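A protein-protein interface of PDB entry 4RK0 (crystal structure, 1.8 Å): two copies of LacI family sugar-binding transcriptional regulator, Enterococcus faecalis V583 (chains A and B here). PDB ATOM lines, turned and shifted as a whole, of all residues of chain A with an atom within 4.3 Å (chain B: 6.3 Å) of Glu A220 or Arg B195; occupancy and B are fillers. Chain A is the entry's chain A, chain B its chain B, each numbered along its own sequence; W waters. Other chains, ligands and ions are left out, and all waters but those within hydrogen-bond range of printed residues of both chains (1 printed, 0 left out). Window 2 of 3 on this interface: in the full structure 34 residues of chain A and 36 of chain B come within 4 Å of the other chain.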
ATOM      1  N   ASP A 217      -9.912 -10.322   0.225  1.00  0.00           N
ATOM      2  CA  ASP A 217      -8.463 -10.577   0.239  1.00  0.00           C
ATOM      3  C   ASP A 217      -8.126 -11.939   0.823  1.00  0.00           C
ATOM      4  O   ASP A 217      -7.209 -12.624   0.336  1.00  0.00           O
ATOM      5  CB  ASP A 217      -7.735  -9.444   0.971  1.00  0.00           C
ATOM      6  CG  ASP A 217      -7.232  -8.375   0.018  1.00  0.00           C
ATOM      7  OD1 ASP A 217      -6.654  -8.739  -1.028  1.00  0.00           O
ATOM      8  OD2 ASP A 217      -7.407  -7.173   0.306  1.00  0.00           O
ATOM      9  N   MET A 218      -8.905 -12.357   1.820  1.00  0.00           N
ATOM     10  CA  MET A 218      -8.733 -13.663   2.465  1.00  0.00           C
ATOM     11  C   MET A 218      -8.812 -14.881   1.540  1.00  0.00           C
ATOM     12  O   MET A 218      -8.411 -15.965   1.956  1.00  0.00           O
ATOM     13  CB  MET A 218      -9.737 -13.875   3.622  1.00  0.00           C
ATOM     14  CG  MET A 218      -9.276 -13.400   5.009  1.00  0.00           C
ATOM     15  SD  MET A 218      -7.643 -13.903   5.594  1.00  0.00           S
ATOM     16  CE  MET A 218      -7.875 -15.477   6.324  1.00  0.00           C
ATOM     17  N   CYS A 219      -9.372 -14.724   0.329  1.00  0.00           N
ATOM     18  CA  CYS A 219      -9.505 -15.854  -0.597  1.00  0.00           C
ATOM     19  C   CYS A 219      -8.155 -16.553  -0.858  1.00  0.00           C
ATOM     20  O   CYS A 219      -8.094 -17.759  -1.072  1.00  0.00           O
ATOM     21  CB  CYS A 219     -10.121 -15.380  -1.902  1.00  0.00           C
ATOM     22  SG  CYS A 219     -11.913 -15.018  -1.774  1.00  0.00           S
ATOM     23  N   GLU A 220      -7.090 -15.762  -0.873  1.00  0.00           N
ATOM     24  CA  GLU A 220      -5.734 -16.264  -1.182  1.00  0.00           C
ATOM     25  C   GLU A 220      -5.008 -16.822   0.050  1.00  0.00           C
ATOM     26  O   GLU A 220      -3.945 -17.402  -0.088  1.00  0.00           O
ATOM     27  CB  GLU A 220      -4.903 -15.144  -1.792  1.00  0.00           C
ATOM     28  CG  GLU A 220      -5.536 -14.492  -3.024  1.00  0.00           C
ATOM     29  CD  GLU A 220      -4.605 -13.570  -3.783  1.00  0.00           C
ATOM     30  OE1 GLU A 220      -3.688 -12.989  -3.169  1.00  0.00           O
ATOM     31  OE2 GLU A 220      -4.814 -13.403  -5.005  1.00  0.00           O
ATOM     32  N   TYR A 221      -5.584 -16.642   1.237  1.00  0.00           N
ATOM     33  CA  TYR A 221      -5.018 -17.122   2.506  1.00  0.00           C
ATOM     34  C   TYR A 221      -5.688 -18.338   3.137  1.00  0.00           C
ATOM     35  O   TYR A 221      -5.193 -18.904   4.107  1.00  0.00           O
ATOM     36  CB  TYR A 221      -4.956 -15.952   3.492  1.00  0.00           C
ATOM     37  CG  TYR A 221      -4.183 -14.840   2.919  1.00  0.00           C
ATOM     38  CD1 TYR A 221      -4.786 -13.846   2.121  1.00  0.00           C
ATOM     39  CD2 TYR A 221      -2.806 -14.771   3.124  1.00  0.00           C
ATOM     40  CE1 TYR A 221      -4.030 -12.817   1.573  1.00  0.00           C
ATOM     41  CE2 TYR A 221      -2.055 -13.766   2.573  1.00  0.00           C
ATOM     42  CZ  TYR A 221      -2.660 -12.783   1.796  1.00  0.00           C
ATOM     43  OH  TYR A 221      -1.835 -11.806   1.278  1.00  0.00           O
ATOM     44  N   VAL A 222      -6.802 -18.774   2.586  1.00  0.00           N
ATOM     45  CA  VAL A 222      -7.419 -20.018   3.009  1.00  0.00           C
ATOM     46  C   VAL A 222      -6.809 -21.180   2.202  1.00  0.00           C
ATOM     47  O   VAL A 222      -6.113 -20.946   1.215  1.00  0.00           O
ATOM     48  CB  VAL A 222      -8.934 -19.948   2.910  1.00  0.00           C
ATOM     49  CG1 VAL A 222      -9.449 -18.958   3.962  1.00  0.00           C
ATOM     50  CG2 VAL A 222      -9.411 -19.518   1.508  1.00  0.00           C
ATOM     51  N   ARG A 267      -8.928 -20.346  -8.757  1.00  0.00           N
ATOM     52  CA  ARG A 267      -7.858 -20.725  -7.851  1.00  0.00           C
ATOM     53  C   ARG A 267      -7.850 -22.229  -7.703  1.00  0.00           C
ATOM     54  O   ARG A 267      -7.771 -22.960  -8.728  1.00  0.00           O
ATOM     55  CB  ARG A 267      -7.975 -19.951  -6.524  1.00  0.00           C
ATOM     56  CG  ARG A 267      -7.772 -18.488  -6.705  1.00  0.00           C
ATOM     57  CD  ARG A 267      -7.494 -17.776  -5.388  1.00  0.00           C
ATOM     58  NE  ARG A 267      -7.242 -16.365  -5.623  1.00  0.00           N
ATOM     59  CZ  ARG A 267      -8.162 -15.390  -5.538  1.00  0.00           C
ATOM     60  NH1 ARG A 267      -9.432 -15.677  -5.264  1.00  0.00           N
ATOM     61  NH2 ARG A 267      -7.815 -14.128  -5.763  1.00  0.00           N
ATOM     62  N   LYS B 164      -1.196  -9.001   5.995  1.00  0.00           N
ATOM     63  CA  LYS B 164      -1.121 -10.301   5.394  1.00  0.00           C
ATOM     64  C   LYS B 164      -0.008 -10.366   4.362  1.00  0.00           C
ATOM     65  O   LYS B 164       0.753 -11.308   4.381  1.00  0.00           O
ATOM     66  CB  LYS B 164      -2.451 -10.693   4.763  1.00  0.00           C
ATOM     67  CG  LYS B 164      -3.575 -10.830   5.784  1.00  0.00           C
ATOM     68  CD  LYS B 164      -4.797 -11.505   5.189  1.00  0.00           C
ATOM     69  CE  LYS B 164      -5.571 -10.587   4.247  1.00  0.00           C
ATOM     70  NZ  LYS B 164      -5.940  -9.292   4.869  1.00  0.00           N
ATOM     71  N   THR B 165       0.107  -9.364   3.472  1.00  0.00           N
ATOM     72  CA  THR B 165       1.160  -9.405   2.457  1.00  0.00           C
ATOM     73  C   THR B 165       2.551  -9.370   3.140  1.00  0.00           C
ATOM     74  O   THR B 165       3.482  -9.972   2.653  1.00  0.00           O
ATOM     75  CB  THR B 165       1.023  -8.248   1.435  1.00  0.00           C
ATOM     76  OG1 THR B 165       0.977  -7.018   2.136  1.00  0.00           O
ATOM     77  CG2 THR B 165      -0.241  -8.384   0.646  1.00  0.00           C
ATOM     78  N   TYR B 168       3.340 -12.848   4.327  1.00  0.00           N
ATOM     79  CA  TYR B 168       3.671 -13.603   3.117  1.00  0.00           C
ATOM     80  C   TYR B 168       5.118 -13.332   2.645  1.00  0.00           C
ATOM     81  O   TYR B 168       5.898 -14.266   2.382  1.00  0.00           O
ATOM     82  CB  TYR B 168       2.698 -13.195   2.013  1.00  0.00           C
ATOM     83  CG  TYR B 168       2.887 -13.907   0.703  1.00  0.00           C
ATOM     84  CD1 TYR B 168       2.697 -15.280   0.590  1.00  0.00           C
ATOM     85  CD2 TYR B 168       3.224 -13.188  -0.439  1.00  0.00           C
ATOM     86  CE1 TYR B 168       2.868 -15.922  -0.641  1.00  0.00           C
ATOM     87  CE2 TYR B 168       3.383 -13.795  -1.651  1.00  0.00           C
ATOM     88  CZ  TYR B 168       3.206 -15.146  -1.769  1.00  0.00           C
ATOM     89  OH  TYR B 168       3.372 -15.689  -3.009  1.00  0.00           O
ATOM     90  N   VAL B 171       8.227 -15.023   4.544  1.00  0.00           N
ATOM     91  CA  VAL B 171       8.474 -16.457   4.555  1.00  0.00           C
ATOM     92  C   VAL B 171       9.826 -16.878   3.975  1.00  0.00           C
ATOM     93  O   VAL B 171      10.489 -17.764   4.528  1.00  0.00           O
ATOM     94  CB  VAL B 171       7.307 -17.231   3.930  1.00  0.00           C
ATOM     95  CG1 VAL B 171       7.636 -18.712   3.834  1.00  0.00           C
ATOM     96  CG2 VAL B 171       6.043 -17.049   4.813  1.00  0.00           C
ATOM     97  N   ALA B 190       0.141 -13.549  10.607  1.00  0.00           N
ATOM     98  CA  ALA B 190       0.131 -15.009  10.682  1.00  0.00           C
ATOM     99  C   ALA B 190      -0.532 -15.620   9.470  1.00  0.00           C
ATOM    100  O   ALA B 190      -0.053 -16.626   8.937  1.00  0.00           O
ATOM    101  CB  ALA B 190      -0.552 -15.478  11.947  1.00  0.00           C
ATOM    102  N   PHE B 191      -1.635 -15.025   9.031  1.00  0.00           N
ATOM    103  CA  PHE B 191      -2.289 -15.503   7.837  1.00  0.00           C
ATOM    104  C   PHE B 191      -1.363 -15.435   6.641  1.00  0.00           C
ATOM    105  O   PHE B 191      -1.359 -16.348   5.821  1.00  0.00           O
ATOM    106  CB  PHE B 191      -3.566 -14.708   7.567  1.00  0.00           C
ATOM    107  CG  PHE B 191      -4.580 -14.757   8.706  1.00  0.00           C
ATOM    108  CD1 PHE B 191      -4.688 -15.876   9.547  1.00  0.00           C
ATOM    109  CD2 PHE B 191      -5.410 -13.692   8.932  1.00  0.00           C
ATOM    110  CE1 PHE B 191      -5.639 -15.915  10.572  1.00  0.00           C
ATOM    111  CE2 PHE B 191      -6.350 -13.726   9.948  1.00  0.00           C
ATOM    112  CZ  PHE B 191      -6.468 -14.821  10.762  1.00  0.00           C
ATOM    113  N   GLY B 192      -0.639 -14.332   6.484  1.00  0.00           N
ATOM    114  CA  GLY B 192       0.433 -14.271   5.503  1.00  0.00           C
ATOM    115  C   GLY B 192       1.435 -15.417   5.591  1.00  0.00           C
ATOM    116  O   GLY B 192       1.792 -15.979   4.581  1.00  0.00           O
ATOM    117  N   LEU B 193       1.867 -15.773   6.808  1.00  0.00           N
ATOM    118  CA  LEU B 193       2.787 -16.878   6.994  1.00  0.00           C
ATOM    119  C   LEU B 193       2.185 -18.165   6.460  1.00  0.00           C
ATOM    120  O   LEU B 193       2.866 -18.937   5.801  1.00  0.00           O
ATOM    121  CB  LEU B 193       3.167 -17.061   8.471  1.00  0.00           C
ATOM    122  CG  LEU B 193       3.904 -15.854   9.064  1.00  0.00           C
ATOM    123  CD1 LEU B 193       4.047 -16.043  10.568  1.00  0.00           C
ATOM    124  CD2 LEU B 193       5.224 -15.567   8.382  1.00  0.00           C
ATOM    125  N   TYR B 194       0.921 -18.417   6.808  1.00  0.00           N
ATOM    126  CA  TYR B 194       0.204 -19.599   6.297  1.00  0.00           C
ATOM    127  C   TYR B 194       0.292 -19.689   4.776  1.00  0.00           C
ATOM    128  O   TYR B 194       0.660 -20.730   4.248  1.00  0.00           O
ATOM    129  CB  TYR B 194      -1.269 -19.588   6.696  1.00  0.00           C
ATOM    130  CG  TYR B 194      -1.615 -20.106   8.085  1.00  0.00           C
ATOM    131  CD1 TYR B 194      -0.871 -19.757   9.216  1.00  0.00           C
ATOM    132  CD2 TYR B 194      -2.754 -20.884   8.282  1.00  0.00           C
ATOM    133  CE1 TYR B 194      -1.242 -20.234  10.482  1.00  0.00           C
ATOM    134  CE2 TYR B 194      -3.111 -21.363   9.535  1.00  0.00           C
ATOM    135  CZ  TYR B 194      -2.366 -21.023  10.637  1.00  0.00           C
ATOM    136  OH  TYR B 194      -2.800 -21.499  11.839  1.00  0.00           O
ATOM    137  N   ARG B 195      -0.086 -18.614   4.079  1.00  0.00           N
ATOM    138  CA  ARG B 195      -0.052 -18.633   2.597  1.00  0.00           C
ATOM    139  C   ARG B 195       1.354 -18.964   2.075  1.00  0.00           C
ATOM    140  O   ARG B 195       1.526 -19.858   1.218  1.00  0.00           O
ATOM    141  CB  ARG B 195      -0.501 -17.293   2.039  1.00  0.00           C
ATOM    142  CG  ARG B 195      -0.524 -17.233   0.515  1.00  0.00           C
ATOM    143  CD  ARG B 195      -0.902 -15.808   0.079  1.00  0.00           C
ATOM    144  NE  ARG B 195      -0.729 -15.651  -1.367  1.00  0.00           N
ATOM    145  CZ  ARG B 195      -0.522 -14.497  -1.990  1.00  0.00           C
ATOM    146  NH1 ARG B 195      -0.483 -13.348  -1.325  1.00  0.00           N
ATOM    147  NH2 ARG B 195      -0.333 -14.504  -3.307  1.00  0.00           N
ATOM    148  N   GLY B 196       2.358 -18.267   2.604  1.00  0.00           N
ATOM    149  CA  GLY B 196       3.721 -18.420   2.142  1.00  0.00           C
ATOM    150  C   GLY B 196       4.291 -19.796   2.430  1.00  0.00           C
ATOM    151  O   GLY B 196       4.959 -20.386   1.580  1.00  0.00           O
ATOM    152  N   LEU B 197       3.999 -20.326   3.621  1.00  0.00           N
ATOM    153  CA  LEU B 197       4.557 -21.598   3.993  1.00  0.00           C
ATOM    154  C   LEU B 197       3.851 -22.699   3.150  1.00  0.00           C
ATOM    155  O   LEU B 197       4.506 -23.646   2.767  1.00  0.00           O
ATOM    156  CB  LEU B 197       4.452 -21.864   5.490  1.00  0.00           C
ATOM    157  CG  LEU B 197       5.336 -20.997   6.397  1.00  0.00           C
ATOM    158  CD1 LEU B 197       4.842 -21.171   7.811  1.00  0.00           C
ATOM    159  CD2 LEU B 197       6.804 -21.442   6.266  1.00  0.00           C
ATOM    160  N   ALA B 198       2.564 -22.528   2.850  1.00  0.00           N
ATOM    161  CA  ALA B 198       1.838 -23.481   1.982  1.00  0.00           C
ATOM    162  C   ALA B 198       2.553 -23.532   0.628  1.00  0.00           C
ATOM    163  O   ALA B 198       2.893 -24.585   0.125  1.00  0.00           O
ATOM    164  CB  ALA B 198       0.378 -23.070   1.819  1.00  0.00           C
ATOM    165  N   GLU B 199       2.826 -22.367   0.069  1.00  0.00           N
ATOM    166  CA  GLU B 199       3.530 -22.267  -1.218  1.00  0.00           C
ATOM    167  C   GLU B 199       4.904 -22.931  -1.216  1.00  0.00           C
ATOM    168  O   GLU B 199       5.288 -23.573  -2.200  1.00  0.00           O
ATOM    169  CB  GLU B 199       3.587 -20.798  -1.671  1.00  0.00           C
ATOM    170  CG  GLU B 199       2.223 -20.311  -2.147  1.00  0.00           C
ATOM    171  CD  GLU B 199       2.208 -18.894  -2.699  1.00  0.00           C
ATOM    172  OE1 GLU B 199       3.277 -18.346  -2.990  1.00  0.00           O
ATOM    173  OE2 GLU B 199       1.103 -18.320  -2.852  1.00  0.00           O
ATOM    174  N   ALA B 200       5.622 -22.848  -0.095  1.00  0.00           N
ATOM    175  CA  ALA B 200       6.928 -23.468   0.006  1.00  0.00           C
ATOM    176  C   ALA B 200       6.888 -24.966   0.323  1.00  0.00           C
ATOM    177  O   ALA B 200       7.915 -25.580   0.505  1.00  0.00           O
ATOM    178  CB  ALA B 200       7.729 -22.737   1.051  1.00  0.00           C
HETATM  179  O   HOH W   1      -2.956 -17.716  -2.526  1.00  0.00           O
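Of the 7 printed residues of chain A, 3 touch a printed residue of chain B.
Hydrophobic or aromatic side chains of chain A that line the printed part of chain B: Met A218 and Tyr A221.
Printed residues of chain B that touch a printed residue of chain A: Lys B164, Thr B165, Phe B191, Gly B192 and Arg B195.
Among the printed residues, 7 pairs touch across the chains.
OE2 of Glu A220 lies within salt-bridge range of NH2 of Arg A267 (3.2 Å).
OE2 of Glu B199 lies within salt-bridge range of NE of Arg B195, at 3.6 Å.
OE1 of Glu A220 lies within salt-bridge range of NH2 of Arg B195.
The guanidinium group of Arg B195 lies within hydrogen-bond range of the side-chain hydroxyl of Tyr A221 (3.3 Å).
Of the printed residues of chain B, Met A218 touches Lys B164 (3.7 Å).
Of chain B, only Arg B195 comes within 4 Å of Glu A220.
Printed residues of chain B within 4 Å of Tyr A221: Lys B164, Thr B165, Phe B191, Gly B192 and Arg B195.
Of the printed residues of chain A, Lys B164 touches Met A218 (3.7 Å) and Tyr A221 (3.6 Å).
Of the printed residues of chain A, Gly B192 touches Tyr A221.
Of the printed residues of chain A, Arg B195 touches Glu A220 and Tyr A221.
Gly B196 touches none of the printed residues of chain A.
The nearest printed residue of chain A that does not touch Arg B195 is Val A222 (6.5 Å).
The nearest printed residue of chain A that does not touch Phe B191 is Met A218 (4.01 Å).
Among the printed residues, merely in contact across the chains: Met A218 with Lys B164 (3.7 Å), Tyr A221 with Lys B164 (3.6 Å), Tyr A221 with Thr B165 (3.8 Å), Tyr A221 with Phe B191 (3.4 Å) and Tyr A221 with Gly B192 (3.9 Å).
Water W1 bridges the backbone carbonyl oxygen (O) of Glu A220 (2.6 Å) and the guanidinium group (NE) of Arg B195 (3.3 Å).
No position is printed for both chains.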
